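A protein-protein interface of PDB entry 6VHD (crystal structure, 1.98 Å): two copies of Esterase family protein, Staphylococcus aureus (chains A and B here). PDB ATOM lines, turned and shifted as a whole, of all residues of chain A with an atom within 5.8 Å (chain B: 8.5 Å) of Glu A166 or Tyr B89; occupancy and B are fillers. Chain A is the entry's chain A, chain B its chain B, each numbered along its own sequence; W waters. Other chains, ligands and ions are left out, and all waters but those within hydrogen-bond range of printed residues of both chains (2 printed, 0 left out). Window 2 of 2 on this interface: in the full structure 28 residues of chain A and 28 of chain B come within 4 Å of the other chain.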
ATOM      1  N   ALA A  88      14.915 -28.970  24.264  1.00  0.00           N
ATOM      2  CA  ALA A  88      16.209 -29.619  24.048  1.00  0.00           C
ATOM      3  C   ALA A  88      17.287 -28.990  24.924  1.00  0.00           C
ATOM      4  O   ALA A  88      18.076 -29.700  25.556  1.00  0.00           O
ATOM      5  CB  ALA A  88      16.616 -29.524  22.575  1.00  0.00           C
ATOM      6  N   TYR A  89      17.345 -27.650  24.955  1.00  0.00           N
ATOM      7  CA  TYR A  89      18.284 -26.881  25.779  1.00  0.00           C
ATOM      8  C   TYR A  89      17.467 -25.837  26.532  1.00  0.00           C
ATOM      9  O   TYR A  89      17.287 -24.717  26.049  1.00  0.00           O
ATOM     10  CB  TYR A  89      19.379 -26.214  24.937  1.00  0.00           C
ATOM     11  CG  TYR A  89      20.026 -27.118  23.933  1.00  0.00           C
ATOM     12  CD1 TYR A  89      19.966 -26.836  22.571  1.00  0.00           C
ATOM     13  CD2 TYR A  89      20.692 -28.269  24.338  1.00  0.00           C
ATOM     14  CE1 TYR A  89      20.570 -27.679  21.630  1.00  0.00           C
ATOM     15  CE2 TYR A  89      21.299 -29.116  23.408  1.00  0.00           C
ATOM     16  CZ  TYR A  89      21.233 -28.816  22.062  1.00  0.00           C
ATOM     17  OH  TYR A  89      21.838 -29.657  21.147  1.00  0.00           O
ATOM     18  N   SER A 164      14.721 -18.355  20.354  1.00  0.00           N
ATOM     19  CA  SER A 164      15.682 -19.391  19.961  1.00  0.00           C
ATOM     20  C   SER A 164      14.946 -20.668  19.565  1.00  0.00           C
ATOM     21  O   SER A 164      14.418 -21.387  20.422  1.00  0.00           O
ATOM     22  CB  SER A 164      16.685 -19.686  21.076  1.00  0.00           C
ATOM     23  OG  SER A 164      17.449 -20.853  20.753  1.00  0.00           O
ATOM     24  N   LYS A 165      14.897 -20.931  18.261  1.00  0.00           N
ATOM     25  CA  LYS A 165      14.364 -22.191  17.760  1.00  0.00           C
ATOM     26  C   LYS A 165      15.108 -23.386  18.349  1.00  0.00           C
ATOM     27  O   LYS A 165      14.488 -24.357  18.794  1.00  0.00           O
ATOM     28  CB  LYS A 165      14.431 -22.207  16.229  1.00  0.00           C
ATOM     29  CG  LYS A 165      14.154 -23.570  15.618  1.00  0.00           C
ATOM     30  CD  LYS A 165      14.337 -23.581  14.112  1.00  0.00           C
ATOM     31  CE  LYS A 165      15.809 -23.615  13.716  1.00  0.00           C
ATOM     32  NZ  LYS A 165      15.959 -24.132  12.334  1.00  0.00           N
ATOM     33  N   GLU A 166      16.451 -23.338  18.339  1.00  0.00           N
ATOM     34  CA  GLU A 166      17.247 -24.501  18.726  1.00  0.00           C
ATOM     35  C   GLU A 166      17.100 -24.838  20.207  1.00  0.00           C
ATOM     36  O   GLU A 166      17.201 -26.010  20.589  1.00  0.00           O
ATOM     37  CB  GLU A 166      18.718 -24.256  18.390  1.00  0.00           C
ATOM     38  CG  GLU A 166      19.023 -24.274  16.903  1.00  0.00           C
ATOM     39  CD  GLU A 166      18.725 -22.944  16.222  1.00  0.00           C
ATOM     40  OE1 GLU A 166      18.231 -22.006  16.895  1.00  0.00           O
ATOM     41  OE2 GLU A 166      18.992 -22.839  15.005  1.00  0.00           O
ATOM     42  N   ALA A 167      16.840 -23.841  21.056  1.00  0.00           N
ATOM     43  CA  ALA A 167      16.572 -24.138  22.461  1.00  0.00           C
ATOM     44  C   ALA A 167      15.395 -25.099  22.599  1.00  0.00           C
ATOM     45  O   ALA A 167      15.419 -26.005  23.443  1.00  0.00           O
ATOM     46  CB  ALA A 167      16.329 -22.846  23.239  1.00  0.00           C
ATOM     47  N   ILE A 168      14.375 -24.957  21.747  1.00  0.00           N
ATOM     48  CA  ILE A 168      13.206 -25.825  21.853  1.00  0.00           C
ATOM     49  C   ILE A 168      13.479 -27.184  21.213  1.00  0.00           C
ATOM     50  O   ILE A 168      13.319 -28.227  21.856  1.00  0.00           O
ATOM     51  CB  ILE A 168      11.965 -25.169  21.222  1.00  0.00           C
ATOM     52  CG1 ILE A 168      11.598 -23.871  21.943  1.00  0.00           C
ATOM     53  CG2 ILE A 168      10.806 -26.176  21.213  1.00  0.00           C
ATOM     54  CD1 ILE A 168      10.669 -22.979  21.147  1.00  0.00           C
ATOM     55  N   ILE A 169      13.866 -27.196  19.932  1.00  0.00           N
ATOM     56  CA  ILE A 169      13.918 -28.434  19.155  1.00  0.00           C
ATOM     57  C   ILE A 169      15.333 -28.952  18.915  1.00  0.00           C
ATOM     58  O   ILE A 169      15.484 -30.023  18.299  1.00  0.00           O
ATOM     59  CB  ILE A 169      13.186 -28.282  17.804  1.00  0.00           C
ATOM     60  CG1 ILE A 169      13.991 -27.363  16.870  1.00  0.00           C
ATOM     61  CG2 ILE A 169      11.743 -27.791  18.021  1.00  0.00           C
ATOM     62  CD1 ILE A 169      13.399 -27.215  15.498  1.00  0.00           C
ATOM     63  N   GLY A 170      16.369 -28.232  19.334  1.00  0.00           N
ATOM     64  CA  GLY A 170      17.718 -28.755  19.140  1.00  0.00           C
ATOM     65  C   GLY A 170      18.157 -28.729  17.685  1.00  0.00           C
ATOM     66  O   GLY A 170      17.920 -27.763  16.954  1.00  0.00           O
ATOM     67  N   ASN A 171      18.815 -29.823  17.270  1.00  0.00           N
ATOM     68  CA  ASN A 171      19.338 -30.079  15.924  1.00  0.00           C
ATOM     69  C   ASN A 171      18.274 -30.329  14.854  1.00  0.00           C
ATOM     70  O   ASN A 171      18.631 -30.370  13.669  1.00  0.00           O
ATOM     71  CB  ASN A 171      20.285 -31.290  15.965  1.00  0.00           C
ATOM     72  CG  ASN A 171      19.575 -32.590  16.369  1.00  0.00           C
ATOM     73  OD1 ASN A 171      18.627 -33.040  15.715  1.00  0.00           O
ATOM     74  ND2 ASN A 171      20.027 -33.189  17.468  1.00  0.00           N
ATOM     75  N   SER B  82      20.260 -18.689  33.500  1.00  0.00           N
ATOM     76  CA  SER B  82      21.105 -18.162  32.432  1.00  0.00           C
ATOM     77  C   SER B  82      22.571 -17.976  32.805  1.00  0.00           C
ATOM     78  O   SER B  82      23.385 -17.742  31.910  1.00  0.00           O
ATOM     79  CB  SER B  82      20.586 -16.803  31.983  1.00  0.00           C
ATOM     80  OG  SER B  82      20.836 -15.855  32.994  1.00  0.00           O
ATOM     81  N   ALA B  85      24.509 -14.774  31.254  1.00  0.00           N
ATOM     82  CA  ALA B  85      25.142 -14.793  29.943  1.00  0.00           C
ATOM     83  C   ALA B  85      24.133 -14.426  28.860  1.00  0.00           C
ATOM     84  O   ALA B  85      22.923 -14.622  29.020  1.00  0.00           O
ATOM     85  CB  ALA B  85      25.716 -16.183  29.646  1.00  0.00           C
ATOM     86  N   ASN B  86      24.640 -13.888  27.753  1.00  0.00           N
ATOM     87  CA  ASN B  86      23.908 -13.922  26.490  1.00  0.00           C
ATOM     88  C   ASN B  86      23.957 -15.362  25.996  1.00  0.00           C
ATOM     89  O   ASN B  86      24.978 -15.819  25.477  1.00  0.00           O
ATOM     90  CB  ASN B  86      24.523 -12.958  25.480  1.00  0.00           C
ATOM     91  CG  ASN B  86      24.300 -11.493  25.868  1.00  0.00           C
ATOM     92  OD1 ASN B  86      23.312 -11.161  26.525  1.00  0.00           O
ATOM     93  ND2 ASN B  86      25.224 -10.614  25.467  1.00  0.00           N
ATOM     94  N   MET B  87      22.849 -16.088  26.152  1.00  0.00           N
ATOM     95  CA  MET B  87      22.876 -17.545  26.039  1.00  0.00           C
ATOM     96  C   MET B  87      23.036 -18.006  24.600  1.00  0.00           C
ATOM     97  O   MET B  87      22.474 -17.418  23.671  1.00  0.00           O
ATOM     98  CB  MET B  87      21.601 -18.156  26.616  1.00  0.00           C
ATOM     99  CG  MET B  87      21.410 -17.881  28.118  1.00  0.00           C
ATOM    100  SD  MET B  87      19.741 -18.238  28.732  1.00  0.00           S
ATOM    101  CE  MET B  87      19.732 -20.036  28.624  1.00  0.00           C
ATOM    102  N   ALA B  88      23.773 -19.107  24.427  1.00  0.00           N
ATOM    103  CA  ALA B  88      23.876 -19.720  23.108  1.00  0.00           C
ATOM    104  C   ALA B  88      22.497 -20.084  22.565  1.00  0.00           C
ATOM    105  O   ALA B  88      22.183 -19.797  21.403  1.00  0.00           O
ATOM    106  CB  ALA B  88      24.775 -20.961  23.172  1.00  0.00           C
ATOM    107  N   TYR B  89      21.666 -20.741  23.387  1.00  0.00           N
ATOM    108  CA  TYR B  89      20.309 -21.148  23.002  1.00  0.00           C
ATOM    109  C   TYR B  89      19.391 -20.679  24.125  1.00  0.00           C
ATOM    110  O   TYR B  89      19.103 -21.438  25.057  1.00  0.00           O
ATOM    111  CB  TYR B  89      20.184 -22.641  22.786  1.00  0.00           C
ATOM    112  CG  TYR B  89      21.216 -23.230  21.845  1.00  0.00           C
ATOM    113  CD1 TYR B  89      22.120 -24.183  22.293  1.00  0.00           C
ATOM    114  CD2 TYR B  89      21.279 -22.836  20.518  1.00  0.00           C
ATOM    115  CE1 TYR B  89      23.060 -24.732  21.438  1.00  0.00           C
ATOM    116  CE2 TYR B  89      22.216 -23.383  19.649  1.00  0.00           C
ATOM    117  CZ  TYR B  89      23.103 -24.326  20.119  1.00  0.00           C
ATOM    118  OH  TYR B  89      24.030 -24.878  19.263  1.00  0.00           O
ATOM    119  N   GLY B  90      18.934 -19.441  24.031  1.00  0.00           N
ATOM    120  CA  GLY B  90      18.127 -18.886  25.102  1.00  0.00           C
ATOM    121  C   GLY B  90      17.948 -17.395  24.933  1.00  0.00           C
ATOM    122  O   GLY B  90      17.671 -16.939  23.820  1.00  0.00           O
ATOM    123  N   HIS B  91      18.098 -16.631  26.020  1.00  0.00           N
ATOM    124  CA  HIS B  91      17.897 -15.193  26.006  1.00  0.00           C
ATOM    125  C   HIS B  91      19.213 -14.459  26.196  1.00  0.00           C
ATOM    126  O   HIS B  91      20.181 -15.002  26.740  1.00  0.00           O
ATOM    127  CB  HIS B  91      16.925 -14.751  27.103  1.00  0.00           C
ATOM    128  CG  HIS B  91      15.532 -15.250  26.910  1.00  0.00           C
ATOM    129  ND1 HIS B  91      14.596 -14.570  26.160  1.00  0.00           N
ATOM    130  CD2 HIS B  91      14.909 -16.356  27.380  1.00  0.00           C
ATOM    131  CE1 HIS B  91      13.454 -15.237  26.177  1.00  0.00           C
ATOM    132  NE2 HIS B  91      13.619 -16.325  26.909  1.00  0.00           N
ATOM    133  N   SER B  92      19.208 -13.185  25.777  1.00  0.00           N
ATOM    134  CA  SER B  92      20.358 -12.285  25.916  1.00  0.00           C
ATOM    135  C   SER B  92      20.354 -11.658  27.314  1.00  0.00           C
ATOM    136  O   SER B  92      20.124 -10.464  27.507  1.00  0.00           O
ATOM    137  CB  SER B  92      20.324 -11.212  24.833  1.00  0.00           C
ATOM    138  OG  SER B  92      20.185 -11.777  23.540  1.00  0.00           O
ATOM    139  N   TYR B  93      20.638 -12.493  28.314  1.00  0.00           N
ATOM    140  CA  TYR B  93      20.479 -12.061  29.698  1.00  0.00           C
ATOM    141  C   TYR B  93      21.623 -11.179  30.193  1.00  0.00           C
ATOM    142  O   TYR B  93      21.406 -10.394  31.125  1.00  0.00           O
ATOM    143  CB  TYR B  93      20.303 -13.278  30.613  1.00  0.00           C
ATOM    144  CG  TYR B  93      18.851 -13.680  30.788  1.00  0.00           C
ATOM    145  CD1 TYR B  93      17.913 -12.769  31.278  1.00  0.00           C
ATOM    146  CD2 TYR B  93      18.409 -14.963  30.457  1.00  0.00           C
ATOM    147  CE1 TYR B  93      16.571 -13.128  31.443  1.00  0.00           C
ATOM    148  CE2 TYR B  93      17.067 -15.338  30.635  1.00  0.00           C
ATOM    149  CZ  TYR B  93      16.157 -14.396  31.118  1.00  0.00           C
ATOM    150  OH  TYR B  93      14.829 -14.724  31.311  1.00  0.00           O
ATOM    151  N   SER B 164      20.487 -26.578  32.229  1.00  0.00           N
ATOM    152  CA  SER B 164      21.083 -26.920  30.935  1.00  0.00           C
ATOM    153  C   SER B 164      22.296 -26.038  30.650  1.00  0.00           C
ATOM    154  O   SER B 164      22.178 -24.859  30.284  1.00  0.00           O
ATOM    155  CB  SER B 164      20.060 -26.869  29.805  1.00  0.00           C
ATOM    156  OG  SER B 164      20.685 -26.800  28.528  1.00  0.00           O
ATOM    157  N   LYS B 165      23.463 -26.647  30.838  1.00  0.00           N
ATOM    158  CA  LYS B 165      24.734 -26.058  30.459  1.00  0.00           C
ATOM    159  C   LYS B 165      24.763 -25.674  28.986  1.00  0.00           C
ATOM    160  O   LYS B 165      25.243 -24.590  28.652  1.00  0.00           O
ATOM    161  CB  LYS B 165      25.807 -27.042  30.903  1.00  0.00           C
ATOM    162  CG  LYS B 165      27.179 -27.019  30.335  1.00  0.00           C
ATOM    163  CD  LYS B 165      27.622 -28.471  30.482  1.00  0.00           C
ATOM    164  CE  LYS B 165      28.450 -29.062  29.375  1.00  0.00           C
ATOM    165  NZ  LYS B 165      29.813 -29.248  29.871  1.00  0.00           N
ATOM    166  N   GLU B 166      24.267 -26.546  28.085  1.00  0.00           N
ATOM    167  CA  GLU B 166      24.362 -26.252  26.652  1.00  0.00           C
ATOM    168  C   GLU B 166      23.540 -25.024  26.268  1.00  0.00           C
ATOM    169  O   GLU B 166      23.911 -24.303  25.331  1.00  0.00           O
ATOM    170  CB  GLU B 166      23.863 -27.430  25.814  1.00  0.00           C
ATOM    171  CG  GLU B 166      24.850 -28.556  25.592  1.00  0.00           C
ATOM    172  CD  GLU B 166      24.755 -29.631  26.647  1.00  0.00           C
ATOM    173  OE1 GLU B 166      24.022 -29.412  27.632  1.00  0.00           O
ATOM    174  OE2 GLU B 166      25.398 -30.696  26.484  1.00  0.00           O
ATOM    175  N   ALA B 167      22.436 -24.755  26.986  1.00  0.00           N
ATOM    176  CA  ALA B 167      21.672 -23.532  26.740  1.00  0.00           C
ATOM    177  C   ALA B 167      22.561 -22.303  26.890  1.00  0.00           C
ATOM    178  O   ALA B 167      22.456 -21.344  26.113  1.00  0.00           O
ATOM    179  CB  ALA B 167      20.478 -23.449  27.702  1.00  0.00           C
ATOM    180  N   ILE B 168      23.469 -22.333  27.867  1.00  0.00           N
ATOM    181  CA  ILE B 168      24.333 -21.189  28.124  1.00  0.00           C
ATOM    182  C   ILE B 168      25.495 -21.154  27.129  1.00  0.00           C
ATOM    183  O   ILE B 168      25.722 -20.135  26.467  1.00  0.00           O
ATOM    184  CB  ILE B 168      24.832 -21.199  29.583  1.00  0.00           C
ATOM    185  CG1 ILE B 168      23.661 -21.133  30.584  1.00  0.00           C
ATOM    186  CG2 ILE B 168      25.715 -19.991  29.841  1.00  0.00           C
ATOM    187  CD1 ILE B 168      24.078 -21.493  31.998  1.00  0.00           C
ATOM    188  N   ILE B 169      26.271 -22.238  27.032  1.00  0.00           N
ATOM    189  CA  ILE B 169      27.552 -22.194  26.312  1.00  0.00           C
ATOM    190  C   ILE B 169      27.555 -22.928  24.959  1.00  0.00           C
ATOM    191  O   ILE B 169      28.600 -22.917  24.283  1.00  0.00           O
ATOM    192  CB  ILE B 169      28.712 -22.707  27.191  1.00  0.00           C
ATOM    193  CG1 ILE B 169      28.605 -24.221  27.425  1.00  0.00           C
ATOM    194  CG2 ILE B 169      28.791 -21.907  28.490  1.00  0.00           C
ATOM    195  CD1 ILE B 169      29.747 -24.797  28.260  1.00  0.00           C
ATOM    196  N   GLY B 170      26.466 -23.590  24.551  1.00  0.00           N
ATOM    197  CA  GLY B 170      26.494 -24.277  23.253  1.00  0.00           C
ATOM    198  C   GLY B 170      27.346 -25.540  23.298  1.00  0.00           C
ATOM    199  O   GLY B 170      27.274 -26.316  24.251  1.00  0.00           O
ATOM    200  N   ASN B 171      28.101 -25.798  22.229  1.00  0.00           N
ATOM    201  CA  ASN B 171      29.065 -26.894  22.152  1.00  0.00           C
ATOM    202  C   ASN B 171      30.365 -26.741  22.966  1.00  0.00           C
ATOM    203  O   ASN B 171      31.159 -27.696  22.990  1.00  0.00           O
ATOM    204  CB  ASN B 171      29.405 -27.241  20.683  1.00  0.00           C
ATOM    205  CG  ASN B 171      29.413 -26.042  19.699  1.00  0.00           C
ATOM    206  OD1 ASN B 171      29.820 -24.892  20.003  1.00  0.00           O
ATOM    207  ND2 ASN B 171      29.304 -26.463  18.418  1.00  0.00           N
ATOM    208  N   LEU B 172      30.643 -25.604  23.606  1.00  0.00           N
ATOM    209  CA  LEU B 172      31.958 -25.446  24.224  1.00  0.00           C
ATOM    210  C   LEU B 172      32.254 -26.578  25.203  1.00  0.00           C
ATOM    211  O   LEU B 172      31.443 -26.893  26.074  1.00  0.00           O
ATOM    212  CB  LEU B 172      32.069 -24.111  24.952  1.00  0.00           C
ATOM    213  CG  LEU B 172      32.074 -23.031  23.888  1.00  0.00           C
ATOM    214  CD1 LEU B 172      31.646 -21.678  24.457  1.00  0.00           C
ATOM    215  CD2 LEU B 172      33.444 -22.987  23.192  1.00  0.00           C
HETATM  216  O   HOH W   1      14.359 -17.556  23.300  1.00  0.00           O
HETATM  217  O   HOH W   2      17.124 -22.075  26.700  1.00  0.00           O
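The backbone carbonyl oxygen of Ala B167 lies within hydrogen-bond range of the backbone NH of Ala B88 (3.1 Å).
N of Ala B167 is in hydrogen-bond range of OG of Ser B164 (3.1 Å).
N of Ala A88 lies within hydrogen-bond range of O of Ala A167 (3.1 Å).
The backbone NH (N) of Tyr B89 is in hydrogen-bond range of the backbone carbonyl oxygen (O) of Ala B167 (2.9 Å).
The backbone carbonyl oxygen (O) of Ala A167 is in hydrogen-bond range of the backbone NH (N) of Tyr A89, 2.9 Å away.
The side-chain hydroxyl of Ser A164 is in hydrogen-bond range of the backbone NH of Ala A167.
Tyr A89 touches Tyr B89 (CD1 to CD1, 3.4 Å).
Tyr A89 touches Ser B164.
Glu B166 touches Tyr A89.
Ala B167 touches Tyr A89.
Tyr B89 touches Ser A164 (CA to OG, 3.7 Å).
N of Gly B90 touches CB of Ser A164, at 3.7 Å.
Glu A166 touches Tyr B89 (CB to CD2, 3.6 Å).
Tyr B89 touches Ala A167 (O to CB, 3.6 Å).
Printed residues of chain B within 4 Å of Tyr A89: Tyr B89 (3.4 Å), Ser B164 (3.7 Å), Glu B166 (3.6 Å) and Ala B167 (3.8 Å).
Glu A166 touches just one residue of chain B: Tyr B89.
Tyr B89 touches just these residues of chain A: Tyr A89 (3.4 Å), Ser A164 (3.7 Å), Glu A166 (3.6 Å) and Ala A167 (3.6 Å).
Of the printed residues of chain A, Gly B90 touches Ser A164.
Of the printed residues of chain A, Glu B166 touches Tyr A89.
Of the printed residues of chain A, Ala B167 touches Tyr A89.
The nearest printed residue of chain A that does not touch Tyr B89 is Ile A168 (6.3 Å).
The nearest printed residue of chain A that does not touch Ala B167 is Ala A167 (6.1 Å).
Printed residues of chain B that touch a printed residue of chain A: Tyr B89, Gly B90, Ser B164, Glu B166 and Ala B167.
Hydrophobic or aromatic side chains of chain B that line the printed part of chain A: Tyr B89 and Ala B167.
Tyr B89 touches its own counterpart, Tyr A89.
Tyr A89 touches Ser B164, and with the chains exchanged Ser A164 touches Tyr B89.
Tyr A89 touches Glu B166, and with the chains exchanged Glu A166 touches Tyr B89.
Tyr A89 touches Ala B167, and with the chains exchanged Ala A167 touches Tyr B89.
10 positions are printed for both chains.
Of the 8 pairs that touch across the chains among the printed residues, 7 have their exchanged pair printed and touching as well.
Water W2 bridges the backbone carbonyl oxygen (O) of Tyr B89 (2.6 Å) and the backbone carbonyl oxygen (O) of Tyr A89 (2.7 Å).
Water W1 bridges the backbone NH (N) of Ser A164 and the backbone carbonyl oxygen (O) of Gly B90.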
